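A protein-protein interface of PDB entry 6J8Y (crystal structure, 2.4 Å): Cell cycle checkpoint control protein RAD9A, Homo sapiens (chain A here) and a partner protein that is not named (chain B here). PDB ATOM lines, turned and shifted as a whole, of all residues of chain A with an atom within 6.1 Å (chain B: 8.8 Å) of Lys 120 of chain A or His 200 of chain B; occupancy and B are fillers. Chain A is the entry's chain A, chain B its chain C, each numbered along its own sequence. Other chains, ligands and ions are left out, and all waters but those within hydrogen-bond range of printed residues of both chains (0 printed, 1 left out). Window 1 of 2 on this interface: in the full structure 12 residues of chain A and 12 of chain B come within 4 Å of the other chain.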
ATOM      1  N   MET A  89      -1.700  -4.175  14.464  1.00  0.00           N
ATOM      2  CA  MET A  89      -2.657  -3.076  14.542  1.00  0.00           C
ATOM      3  C   MET A  89      -2.287  -1.966  13.560  1.00  0.00           C
ATOM      4  O   MET A  89      -3.159  -1.367  12.929  1.00  0.00           O
ATOM      5  CB  MET A  89      -2.729  -2.524  15.969  1.00  0.00           C
ATOM      6  CG  MET A  89      -3.171  -1.069  16.057  1.00  0.00           C
ATOM      7  SD  MET A  89      -3.443  -0.507  17.747  1.00  0.00           S
ATOM      8  CE  MET A  89      -3.513   1.266  17.506  1.00  0.00           C
ATOM      9  N   VAL A 110       1.820  12.279  18.815  1.00  0.00           N
ATOM     10  CA  VAL A 110       1.734  11.239  17.799  1.00  0.00           C
ATOM     11  C   VAL A 110       0.282  10.837  17.577  1.00  0.00           C
ATOM     12  O   VAL A 110      -0.357  10.270  18.465  1.00  0.00           O
ATOM     13  CB  VAL A 110       2.551   9.992  18.184  1.00  0.00           C
ATOM     14  CG1 VAL A 110       2.544   8.987  17.043  1.00  0.00           C
ATOM     15  CG2 VAL A 110       3.975  10.380  18.547  1.00  0.00           C
ATOM     16  N   GLN A 111      -0.239  11.141  16.394  1.00  0.00           N
ATOM     17  CA  GLN A 111      -1.605  10.776  16.045  1.00  0.00           C
ATOM     18  C   GLN A 111      -1.646   9.585  15.099  1.00  0.00           C
ATOM     19  O   GLN A 111      -0.938   9.552  14.092  1.00  0.00           O
ATOM     20  CB  GLN A 111      -2.341  11.953  15.405  1.00  0.00           C
ATOM     21  CG  GLN A 111      -2.831  13.004  16.382  1.00  0.00           C
ATOM     22  CD  GLN A 111      -3.780  13.991  15.731  1.00  0.00           C
ATOM     23  OE1 GLN A 111      -4.405  13.688  14.715  1.00  0.00           O
ATOM     24  NE2 GLN A 111      -3.892  15.179  16.313  1.00  0.00           N
ATOM     25  N   LEU A 112      -2.480   8.608  15.429  1.00  0.00           N
ATOM     26  CA  LEU A 112      -2.743   7.497  14.529  1.00  0.00           C
ATOM     27  C   LEU A 112      -4.137   7.648  13.935  1.00  0.00           C
ATOM     28  O   LEU A 112      -5.137   7.562  14.647  1.00  0.00           O
ATOM     29  CB  LEU A 112      -2.610   6.159  15.258  1.00  0.00           C
ATOM     30  CG  LEU A 112      -1.267   5.886  15.939  1.00  0.00           C
ATOM     31  CD1 LEU A 112      -1.257   4.504  16.570  1.00  0.00           C
ATOM     32  CD2 LEU A 112      -0.120   6.036  14.954  1.00  0.00           C
ATOM     33  N   HIS A 113      -4.196   7.900  12.632  1.00  0.00           N
ATOM     34  CA  HIS A 113      -5.470   7.985  11.929  1.00  0.00           C
ATOM     35  C   HIS A 113      -5.883   6.592  11.476  1.00  0.00           C
ATOM     36  O   HIS A 113      -5.286   6.023  10.562  1.00  0.00           O
ATOM     37  CB  HIS A 113      -5.372   8.944  10.741  1.00  0.00           C
ATOM     38  CG  HIS A 113      -5.067  10.357  11.131  1.00  0.00           C
ATOM     39  ND1 HIS A 113      -6.039  11.241  11.547  1.00  0.00           N
ATOM     40  CD2 HIS A 113      -3.897  11.036  11.177  1.00  0.00           C
ATOM     41  CE1 HIS A 113      -5.481  12.405  11.829  1.00  0.00           C
ATOM     42  NE2 HIS A 113      -4.182  12.307  11.612  1.00  0.00           N
ATOM     43  N   CYS A 114      -6.904   6.045  12.126  1.00  0.00           N
ATOM     44  CA  CYS A 114      -7.272   4.650  11.930  1.00  0.00           C
ATOM     45  C   CYS A 114      -8.579   4.491  11.160  1.00  0.00           C
ATOM     46  O   CYS A 114      -9.267   5.471  10.873  1.00  0.00           O
ATOM     47  CB  CYS A 114      -7.376   3.943  13.282  1.00  0.00           C
ATOM     48  SG  CYS A 114      -5.908   4.132  14.326  1.00  0.00           S
ATOM     49  N   VAL A 118     -11.630   6.296  13.461  1.00  0.00           N
ATOM     50  CA  VAL A 118     -11.023   6.209  14.785  1.00  0.00           C
ATOM     51  C   VAL A 118      -9.676   6.927  14.807  1.00  0.00           C
ATOM     52  O   VAL A 118      -8.870   6.781  13.889  1.00  0.00           O
ATOM     53  CB  VAL A 118     -10.835   4.746  15.225  1.00  0.00           C
ATOM     54  CG1 VAL A 118     -10.266   4.679  16.634  1.00  0.00           C
ATOM     55  CG2 VAL A 118     -12.156   4.004  15.149  1.00  0.00           C
ATOM     56  N   ARG A 119      -9.441   7.708  15.857  1.00  0.00           N
ATOM     57  CA  ARG A 119      -8.205   8.469  15.981  1.00  0.00           C
ATOM     58  C   ARG A 119      -7.569   8.269  17.354  1.00  0.00           C
ATOM     59  O   ARG A 119      -8.200   8.518  18.381  1.00  0.00           O
ATOM     60  CB  ARG A 119      -8.471   9.953  15.725  1.00  0.00           C
ATOM     61  CG  ARG A 119      -7.243  10.842  15.817  1.00  0.00           C
ATOM     62  CD  ARG A 119      -7.522  12.211  15.218  1.00  0.00           C
ATOM     63  NE  ARG A 119      -7.636  13.250  16.236  1.00  0.00           N
ATOM     64  CZ  ARG A 119      -8.056  14.487  15.994  1.00  0.00           C
ATOM     65  NH1 ARG A 119      -8.408  14.841  14.765  1.00  0.00           N
ATOM     66  NH2 ARG A 119      -8.128  15.370  16.981  1.00  0.00           N
ATOM     67  N   LYS A 120      -6.321   7.811  17.368  1.00  0.00           N
ATOM     68  CA  LYS A 120      -5.598   7.610  18.620  1.00  0.00           C
ATOM     69  C   LYS A 120      -4.486   8.642  18.772  1.00  0.00           C
ATOM     70  O   LYS A 120      -3.623   8.773  17.904  1.00  0.00           O
ATOM     71  CB  LYS A 120      -5.022   6.195  18.691  1.00  0.00           C
ATOM     72  CG  LYS A 120      -4.751   5.722  20.109  1.00  0.00           C
ATOM     73  CD  LYS A 120      -4.047   4.377  20.132  1.00  0.00           C
ATOM     74  CE  LYS A 120      -4.153   3.735  21.505  1.00  0.00           C
ATOM     75  NZ  LYS A 120      -4.011   4.739  22.597  1.00  0.00           N
ATOM     76  N   THR A 121      -4.508   9.371  19.883  1.00  0.00           N
ATOM     77  CA  THR A 121      -3.544  10.438  20.118  1.00  0.00           C
ATOM     78  C   THR A 121      -2.658  10.145  21.325  1.00  0.00           C
ATOM     79  O   THR A 121      -3.153   9.884  22.421  1.00  0.00           O
ATOM     80  CB  THR A 121      -4.252  11.792  20.332  1.00  0.00           C
ATOM     81  OG1 THR A 121      -4.872  12.206  19.109  1.00  0.00           O
ATOM     82  CG2 THR A 121      -3.257  12.856  20.771  1.00  0.00           C
ATOM     83  N   HIS A 122      -1.347  10.185  21.111  1.00  0.00           N
ATOM     84  CA  HIS A 122      -0.382  10.007  22.190  1.00  0.00           C
ATOM     85  C   HIS A 122       0.379  11.301  22.451  1.00  0.00           C
ATOM     86  O   HIS A 122       1.028  11.841  21.555  1.00  0.00           O
ATOM     87  CB  HIS A 122       0.608   8.887  21.859  1.00  0.00           C
ATOM     88  CG  HIS A 122      -0.032   7.550  21.649  1.00  0.00           C
ATOM     89  ND1 HIS A 122      -0.332   6.698  22.689  1.00  0.00           N
ATOM     90  CD2 HIS A 122      -0.416   6.916  20.517  1.00  0.00           C
ATOM     91  CE1 HIS A 122      -0.880   5.596  22.206  1.00  0.00           C
ATOM     92  NE2 HIS A 122      -0.943   5.703  20.891  1.00  0.00           N
ATOM     93  N   ASN A 123       0.296  11.799  23.679  1.00  0.00           N
ATOM     94  CA  ASN A 123       1.047  12.984  24.068  1.00  0.00           C
ATOM     95  C   ASN A 123       2.286  12.592  24.863  1.00  0.00           C
ATOM     96  O   ASN A 123       2.223  12.384  26.075  1.00  0.00           O
ATOM     97  CB  ASN A 123       0.166  13.938  24.873  1.00  0.00           C
ATOM     98  CG  ASN A 123      -1.015  14.453  24.072  1.00  0.00           C
ATOM     99  OD1 ASN A 123      -0.844  15.024  22.995  1.00  0.00           O
ATOM    100  ND2 ASN A 123      -2.220  14.241  24.587  1.00  0.00           N
ATOM    101  N   GLU B 165      -8.764  -4.567  19.608  1.00  0.00           N
ATOM    102  CA  GLU B 165      -7.361  -4.177  19.389  1.00  0.00           C
ATOM    103  C   GLU B 165      -6.921  -3.099  20.371  1.00  0.00           C
ATOM    104  O   GLU B 165      -5.827  -3.133  20.929  1.00  0.00           O
ATOM    105  CB  GLU B 165      -7.161  -3.635  17.956  1.00  0.00           C
ATOM    106  CG  GLU B 165      -8.284  -3.985  17.007  1.00  0.00           C
ATOM    107  CD  GLU B 165      -9.556  -3.233  17.331  1.00  0.00           C
ATOM    108  OE1 GLU B 165      -9.586  -1.985  17.506  1.00  0.00           O
ATOM    109  OE2 GLU B 165     -10.558  -3.942  17.528  1.00  0.00           O
ATOM    110  N   ALA B 166      -7.810  -2.140  20.582  1.00  0.00           N
ATOM    111  CA  ALA B 166      -7.457  -0.912  21.264  1.00  0.00           C
ATOM    112  C   ALA B 166      -7.407  -1.018  22.785  1.00  0.00           C
ATOM    113  O   ALA B 166      -6.469  -0.524  23.400  1.00  0.00           O
ATOM    114  CB  ALA B 166      -8.412   0.168  20.862  1.00  0.00           C
ATOM    115  N   PHE B 167      -8.404  -1.659  23.387  1.00  0.00           N
ATOM    116  CA  PHE B 167      -8.535  -1.663  24.842  1.00  0.00           C
ATOM    117  C   PHE B 167      -7.720  -2.766  25.515  1.00  0.00           C
ATOM    118  O   PHE B 167      -7.533  -2.756  26.731  1.00  0.00           O
ATOM    119  CB  PHE B 167     -10.008  -1.783  25.237  1.00  0.00           C
ATOM    120  CG  PHE B 167     -10.925  -0.939  24.404  1.00  0.00           C
ATOM    121  CD1 PHE B 167     -10.790   0.438  24.381  1.00  0.00           C
ATOM    122  CD2 PHE B 167     -11.936  -1.514  23.664  1.00  0.00           C
ATOM    123  CE1 PHE B 167     -11.635   1.218  23.617  1.00  0.00           C
ATOM    124  CE2 PHE B 167     -12.785  -0.739  22.908  1.00  0.00           C
ATOM    125  CZ  PHE B 167     -12.634   0.627  22.879  1.00  0.00           C
ATOM    126  N   SER B 168      -7.227  -3.710  24.720  1.00  0.00           N
ATOM    127  CA  SER B 168      -6.201  -4.629  25.199  1.00  0.00           C
ATOM    128  C   SER B 168      -4.857  -3.920  25.109  1.00  0.00           C
ATOM    129  O   SER B 168      -3.826  -4.444  25.537  1.00  0.00           O
ATOM    130  CB  SER B 168      -6.183  -5.927  24.389  1.00  0.00           C
ATOM    131  OG  SER B 168      -7.493  -6.385  24.103  1.00  0.00           O
ATOM    132  N   GLU B 169      -4.894  -2.714  24.553  1.00  0.00           N
ATOM    133  CA  GLU B 169      -3.705  -1.909  24.312  1.00  0.00           C
ATOM    134  C   GLU B 169      -3.732  -0.609  25.130  1.00  0.00           C
ATOM    135  O   GLU B 169      -2.811   0.202  25.049  1.00  0.00           O
ATOM    136  CB  GLU B 169      -3.581  -1.606  22.810  1.00  0.00           C
ATOM    137  CG  GLU B 169      -2.256  -0.991  22.372  1.00  0.00           C
ATOM    138  CD  GLU B 169      -1.459  -1.884  21.445  1.00  0.00           C
ATOM    139  OE1 GLU B 169      -1.766  -3.091  21.358  1.00  0.00           O
ATOM    140  OE2 GLU B 169      -0.515  -1.374  20.807  1.00  0.00           O
ATOM    141  N   LEU B 170      -4.781  -0.409  25.924  1.00  0.00           N
ATOM    142  CA  LEU B 170      -4.878   0.804  26.737  1.00  0.00           C
ATOM    143  C   LEU B 170      -3.836   0.810  27.853  1.00  0.00           C
ATOM    144  O   LEU B 170      -3.596  -0.212  28.499  1.00  0.00           O
ATOM    145  CB  LEU B 170      -6.286   0.965  27.321  1.00  0.00           C
ATOM    146  CG  LEU B 170      -7.144   2.047  26.652  1.00  0.00           C
ATOM    147  CD1 LEU B 170      -7.215   1.847  25.155  1.00  0.00           C
ATOM    148  CD2 LEU B 170      -8.546   2.096  27.236  1.00  0.00           C
ATOM    149  N   ASP B 171      -3.218   1.971  28.059  1.00  0.00           N
ATOM    150  CA  ASP B 171      -2.152   2.142  29.043  1.00  0.00           C
ATOM    151  C   ASP B 171      -2.590   1.687  30.432  1.00  0.00           C
ATOM    152  O   ASP B 171      -3.604   2.148  30.956  1.00  0.00           O
ATOM    153  CB  ASP B 171      -1.703   3.606  29.086  1.00  0.00           C
ATOM    154  CG  ASP B 171      -0.384   3.796  29.812  1.00  0.00           C
ATOM    155  OD1 ASP B 171       0.126   2.820  30.403  1.00  0.00           O
ATOM    156  OD2 ASP B 171       0.143   4.928  29.795  1.00  0.00           O
ATOM    157  N   LEU B 177      -9.211   5.240  34.003  1.00  0.00           N
ATOM    158  CA  LEU B 177      -9.707   5.299  32.637  1.00  0.00           C
ATOM    159  C   LEU B 177     -10.804   6.352  32.576  1.00  0.00           C
ATOM    160  O   LEU B 177     -11.844   6.214  33.219  1.00  0.00           O
ATOM    161  CB  LEU B 177     -10.235   3.942  32.173  1.00  0.00           C
ATOM    162  CG  LEU B 177     -10.937   3.948  30.812  1.00  0.00           C
ATOM    163  CD1 LEU B 177      -9.997   4.430  29.716  1.00  0.00           C
ATOM    164  CD2 LEU B 177     -11.492   2.571  30.482  1.00  0.00           C
ATOM    165  N   GLN B 178     -10.562   7.411  31.815  1.00  0.00           N
ATOM    166  CA  GLN B 178     -11.518   8.504  31.716  1.00  0.00           C
ATOM    167  C   GLN B 178     -12.368   8.375  30.459  1.00  0.00           C
ATOM    168  O   GLN B 178     -11.850   8.381  29.342  1.00  0.00           O
ATOM    169  CB  GLN B 178     -10.794   9.850  31.732  1.00  0.00           C
ATOM    170  CG  GLN B 178     -11.717  11.045  31.599  1.00  0.00           C
ATOM    171  CD  GLN B 178     -10.984  12.363  31.729  1.00  0.00           C
ATOM    172  OE1 GLN B 178     -10.507  12.718  32.807  1.00  0.00           O
ATOM    173  NE2 GLN B 178     -10.886  13.097  30.627  1.00  0.00           N
ATOM    174  N   THR B 180     -15.220   9.978  28.109  1.00  0.00           N
ATOM    175  CA  THR B 180     -15.967  11.168  27.734  1.00  0.00           C
ATOM    176  C   THR B 180     -17.067  10.808  26.745  1.00  0.00           C
ATOM    177  O   THR B 180     -16.813  10.173  25.722  1.00  0.00           O
ATOM    178  CB  THR B 180     -15.058  12.247  27.112  1.00  0.00           C
ATOM    179  OG1 THR B 180     -14.076  12.660  28.070  1.00  0.00           O
ATOM    180  CG2 THR B 180     -15.879  13.456  26.684  1.00  0.00           C
ATOM    181  N   PRO B 186     -15.389  15.317  21.126  1.00  0.00           N
ATOM    182  CA  PRO B 186     -15.047  14.208  20.229  1.00  0.00           C
ATOM    183  C   PRO B 186     -16.040  13.044  20.262  1.00  0.00           C
ATOM    184  O   PRO B 186     -15.657  11.927  19.910  1.00  0.00           O
ATOM    185  CB  PRO B 186     -13.691  13.756  20.763  1.00  0.00           C
ATOM    186  CG  PRO B 186     -13.816  13.969  22.236  1.00  0.00           C
ATOM    187  CD  PRO B 186     -14.700  15.189  22.423  1.00  0.00           C
ATOM    188  N   PHE B 188     -17.158  10.337  21.462  1.00  0.00           N
ATOM    189  CA  PHE B 188     -16.843   9.264  22.402  1.00  0.00           C
ATOM    190  C   PHE B 188     -15.334   9.094  22.552  1.00  0.00           C
ATOM    191  O   PHE B 188     -14.634   8.810  21.581  1.00  0.00           O
ATOM    192  CB  PHE B 188     -17.481   7.946  21.956  1.00  0.00           C
ATOM    193  CG  PHE B 188     -17.216   6.799  22.891  1.00  0.00           C
ATOM    194  CD1 PHE B 188     -17.401   6.948  24.256  1.00  0.00           C
ATOM    195  CD2 PHE B 188     -16.786   5.575  22.408  1.00  0.00           C
ATOM    196  CE1 PHE B 188     -17.159   5.898  25.123  1.00  0.00           C
ATOM    197  CE2 PHE B 188     -16.542   4.520  23.271  1.00  0.00           C
ATOM    198  CZ  PHE B 188     -16.728   4.683  24.629  1.00  0.00           C
ATOM    199  N   ARG B 189     -14.839   9.255  23.776  1.00  0.00           N
ATOM    200  CA  ARG B 189     -13.400   9.249  24.016  1.00  0.00           C
ATOM    201  C   ARG B 189     -12.974   8.470  25.260  1.00  0.00           C
ATOM    202  O   ARG B 189     -13.498   8.686  26.354  1.00  0.00           O
ATOM    203  CB  ARG B 189     -12.886  10.686  24.123  1.00  0.00           C
ATOM    204  CG  ARG B 189     -11.521  10.800  24.780  1.00  0.00           C
ATOM    205  CD  ARG B 189     -11.001  12.223  24.737  1.00  0.00           C
ATOM    206  NE  ARG B 189     -10.607  12.612  23.387  1.00  0.00           N
ATOM    207  CZ  ARG B 189     -10.025  13.767  23.085  1.00  0.00           C
ATOM    208  NH1 ARG B 189      -9.768  14.651  24.039  1.00  0.00           N
ATOM    209  NH2 ARG B 189      -9.697  14.037  21.828  1.00  0.00           N
ATOM    210  N   LEU B 190     -12.013   7.569  25.077  1.00  0.00           N
ATOM    211  CA  LEU B 190     -11.354   6.892  26.188  1.00  0.00           C
ATOM    212  C   LEU B 190      -9.967   7.495  26.394  1.00  0.00           C
ATOM    213  O   LEU B 190      -9.162   7.540  25.464  1.00  0.00           O
ATOM    214  CB  LEU B 190     -11.240   5.385  25.936  1.00  0.00           C
ATOM    215  CG  LEU B 190     -12.515   4.554  25.758  1.00  0.00           C
ATOM    216  CD1 LEU B 190     -13.623   5.053  26.673  1.00  0.00           C
ATOM    217  CD2 LEU B 190     -12.969   4.530  24.305  1.00  0.00           C
ATOM    218  N   SER B 191      -9.689   7.956  27.608  1.00  0.00           N
ATOM    219  CA  SER B 191      -8.412   8.600  27.896  1.00  0.00           C
ATOM    220  C   SER B 191      -7.674   7.939  29.055  1.00  0.00           C
ATOM    221  O   SER B 191      -8.278   7.576  30.065  1.00  0.00           O
ATOM    222  CB  SER B 191      -8.621  10.085  28.199  1.00  0.00           C
ATOM    223  OG  SER B 191      -9.235  10.748  27.109  1.00  0.00           O
ATOM    224  N   THR B 192      -6.363   7.788  28.899  1.00  0.00           N
ATOM    225  CA  THR B 192      -5.511   7.277  29.964  1.00  0.00           C
ATOM    226  C   THR B 192      -4.407   8.283  30.269  1.00  0.00           C
ATOM    227  O   THR B 192      -4.070   9.118  29.428  1.00  0.00           O
ATOM    228  CB  THR B 192      -4.880   5.917  29.597  1.00  0.00           C
ATOM    229  OG1 THR B 192      -4.070   6.062  28.424  1.00  0.00           O
ATOM    230  CG2 THR B 192      -5.961   4.879  29.337  1.00  0.00           C
ATOM    231  N   PHE B 193      -3.854   8.208  31.474  1.00  0.00           N
ATOM    232  CA  PHE B 193      -2.792   9.121  31.878  1.00  0.00           C
ATOM    233  C   PHE B 193      -1.667   8.382  32.594  1.00  0.00           C
ATOM    234  O   PHE B 193      -1.603   8.371  33.823  1.00  0.00           O
ATOM    235  CB  PHE B 193      -3.345  10.227  32.780  1.00  0.00           C
ATOM    236  CG  PHE B 193      -4.530  10.949  32.204  1.00  0.00           C
ATOM    237  CD1 PHE B 193      -5.818  10.509  32.462  1.00  0.00           C
ATOM    238  CD2 PHE B 193      -4.356  12.068  31.406  1.00  0.00           C
ATOM    239  CE1 PHE B 193      -6.911  11.169  31.934  1.00  0.00           C
ATOM    240  CE2 PHE B 193      -5.444  12.733  30.875  1.00  0.00           C
ATOM    241  CZ  PHE B 193      -6.724  12.282  31.141  1.00  0.00           C
ATOM    242  N   GLY B 197       2.868  10.388  29.578  1.00  0.00           N
ATOM    243  CA  GLY B 197       2.013   9.945  28.494  1.00  0.00           C
ATOM    244  C   GLY B 197       0.530  10.209  28.675  1.00  0.00           C
ATOM    245  O   GLY B 197      -0.145   9.535  29.454  1.00  0.00           O
ATOM    246  N   SER B 198       0.025  11.202  27.951  1.00  0.00           N
ATOM    247  CA  SER B 198      -1.411  11.409  27.828  1.00  0.00           C
ATOM    248  C   SER B 198      -1.888  10.710  26.560  1.00  0.00           C
ATOM    249  O   SER B 198      -1.390  10.986  25.469  1.00  0.00           O
ATOM    250  CB  SER B 198      -1.749  12.900  27.789  1.00  0.00           C
ATOM    251  OG  SER B 198      -3.076  13.113  27.340  1.00  0.00           O
ATOM    252  N   SER B 199      -2.845   9.798  26.702  1.00  0.00           N
ATOM    253  CA  SER B 199      -3.290   8.989  25.573  1.00  0.00           C
ATOM    254  C   SER B 199      -4.805   9.042  25.379  1.00  0.00           C
ATOM    255  O   SER B 199      -5.568   8.758  26.302  1.00  0.00           O
ATOM    256  CB  SER B 199      -2.837   7.539  25.756  1.00  0.00           C
ATOM    257  OG  SER B 199      -3.141   6.759  24.614  1.00  0.00           O
ATOM    258  N   HIS B 200      -5.232   9.397  24.171  1.00  0.00           N
ATOM    259  CA  HIS B 200      -6.653   9.536  23.871  1.00  0.00           C
ATOM    260  C   HIS B 200      -7.108   8.585  22.771  1.00  0.00           C
ATOM    261  O   HIS B 200      -6.399   8.360  21.792  1.00  0.00           O
ATOM    262  CB  HIS B 200      -6.975  10.976  23.464  1.00  0.00           C
ATOM    263  CG  HIS B 200      -6.613  11.993  24.499  1.00  0.00           C
ATOM    264  ND1 HIS B 200      -7.186  12.015  25.752  1.00  0.00           N
ATOM    265  CD2 HIS B 200      -5.740  13.026  24.466  1.00  0.00           C
ATOM    266  CE1 HIS B 200      -6.679  13.018  26.448  1.00  0.00           C
ATOM    267  NE2 HIS B 200      -5.799  13.648  25.689  1.00  0.00           N
ATOM    268  N   LEU B 201      -8.307   8.037  22.940  1.00  0.00           N
ATOM    269  CA  LEU B 201      -8.909   7.165  21.942  1.00  0.00           C
ATOM    270  C   LEU B 201     -10.282   7.705  21.556  1.00  0.00           C
ATOM    271  O   LEU B 201     -11.207   7.689  22.364  1.00  0.00           O
ATOM    272  CB  LEU B 201      -9.018   5.742  22.479  1.00  0.00           C
ATOM    273  CG  LEU B 201      -9.305   4.630  21.478  1.00  0.00           C
ATOM    274  CD1 LEU B 201      -8.346   4.696  20.302  1.00  0.00           C
ATOM    275  CD2 LEU B 201      -9.184   3.306  22.192  1.00  0.00           C
ATOM    276  N   ASP B 202     -10.410   8.187  20.325  1.00  0.00           N
ATOM    277  CA  ASP B 202     -11.622   8.885  19.908  1.00  0.00           C
ATOM    278  C   ASP B 202     -12.438   8.125  18.867  1.00  0.00           C
ATOM    279  O   ASP B 202     -11.899   7.619  17.881  1.00  0.00           O
ATOM    280  CB  ASP B 202     -11.270  10.271  19.365  1.00  0.00           C
ATOM    281  CG  ASP B 202     -10.629  11.158  20.412  1.00  0.00           C
ATOM    282  OD1 ASP B 202     -10.754  10.844  21.614  1.00  0.00           O
ATOM    283  OD2 ASP B 202     -10.004  12.171  20.036  1.00  0.00           O
ATOM    284  N   TYR B 203     -13.745   8.061  19.100  1.00  0.00           N
ATOM    285  CA  TYR B 203     -14.683   7.457  18.162  1.00  0.00           C
ATOM    286  C   TYR B 203     -15.758   8.465  17.767  1.00  0.00           C
ATOM    287  O   TYR B 203     -16.523   8.922  18.616  1.00  0.00           O
ATOM    288  CB  TYR B 203     -15.338   6.214  18.770  1.00  0.00           C
ATOM    289  CG  TYR B 203     -14.384   5.074  19.048  1.00  0.00           C
ATOM    290  CD1 TYR B 203     -13.680   5.006  20.243  1.00  0.00           C
ATOM    291  CD2 TYR B 203     -14.198   4.060  18.119  1.00  0.00           C
ATOM    292  CE1 TYR B 203     -12.809   3.963  20.501  1.00  0.00           C
ATOM    293  CE2 TYR B 203     -13.330   3.018  18.366  1.00  0.00           C
ATOM    294  CZ  TYR B 203     -12.641   2.971  19.559  1.00  0.00           C
ATOM    295  OH  TYR B 203     -11.777   1.928  19.806  1.00  0.00           O
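The backbone NH (N) of Asn 123 of chain A sits at hydrogen-bond distance from the backbone carbonyl oxygen (O) of Ser 198 of chain B (2.6 Å). OG of Ser 199 of chain B is in hydrogen-bond range of NZ of Lys 120 of chain A (3.0 Å). A ring nitrogen (ND1) of His 122 of chain A sits at hydrogen-bond distance from the side-chain hydroxyl of Ser 199 of chain B. The backbone carbonyl oxygen of Thr 121 of chain A lies within hydrogen-bond range of the backbone NH of His 200 of chain B (2.8 Å). The backbone NH of Asp 202 of chain B is in hydrogen-bond range of the backbone carbonyl oxygen of Arg 119 of chain A, 3.0 Å away.
The backbone carbonyl oxygen (O) of Leu 190 of chain B sits at hydrogen-bond distance from the backbone NH (N) of Leu 201 of chain B (2.7 Å). N of His 122 of chain A sits at hydrogen-bond distance from O of Val 110 of chain A, 2.8 Å away. The backbone carbonyl oxygen (O) of Phe 188 of chain B sits at hydrogen-bond distance from the backbone NH (N) of Tyr 203 of chain B (2.7 Å). O of Ser 199 of chain B sits at hydrogen-bond distance from N of Thr 192 of chain B (2.9 Å). A ring nitrogen (NE2) of His 200 of chain B lies within hydrogen-bond range of the side-chain hydroxyl of Ser 198 of chain B (3.2 Å). The guanidinium group (NE) of Arg 189 of chain B is in salt-bridge range of the side-chain carboxylate (OD1) of Asp 202 of chain B (2.5 Å).
Of the 12 printed residues of chain A, 6 touch a printed residue of chain B. Hydrophobic or aromatic side chains of chain A within 4 Å of the printed part of chain B: Val 118 and His 122. Of the 24 printed residues of chain B, 7 touch a printed residue of chain A. Printed residues of chain B that touch a printed residue of chain A: Gly 197, Ser 198, Ser 199, His 200, Leu 201, Asp 202 and Tyr 203. Hydrophobic or aromatic side chains of chain B within 4 Å of the printed part of chain A: His 200, Leu 201 and Tyr 203. Among the printed residues, 16 pairs touch across the chains.
Of chain B, only Ser 199, His 200 and Leu 201 come within 4 Å of Lys 120 of chain A. His 200 of chain B touches just these residues of chain A: Arg 119, Lys 120, Thr 121 and Asn 123. Thr 121 of chain A touches three residues of chain B. Printed residues of chain A within 4 Å of Tyr 203 of chain B: Val 118 (3.6 Å). Of the printed residues of chain A, Ser 198 of chain B touches Thr 121, His 122 and Asn 123. Of the printed residues of chain A, Asp 202 of chain B touches Val 118 and Arg 119. Printed residues of chain A within 4 Å of Gly 197 of chain B: Asn 123 (3.4 Å). The nearest residue of chain B that does not touch Lys 120 of chain A is Leu 170 of chain B (5.0 Å). The nearest printed residue of chain B that does not touch Asn 123 of chain A is Ser 199 of chain B (4.8 Å).
Tyr 203 of chain B touches Val 118 of chain A. O of His 200 of chain B touches O of Arg 119 of chain A, at 3.9 Å. Leu 201 of chain B touches Arg 119 of chain A. Lys 120 of chain A touches His 200 of chain B (CA to O, 3.4 Å). Lys 120 of chain A touches Leu 201 of chain B (CG to CD1, 3.7 Å). Thr 121 of chain A touches Ser 198 of chain B (O to O, 3.7 Å). Ser 199 of chain B touches Thr 121 of chain A. O of Ser 198 of chain B touches C of His 122 of chain A, 3.5 Å away. O of Asn 123 of chain A touches CA of Gly 197 of chain B (3.4 Å). Asn 123 of chain A touches His 200 of chain B.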
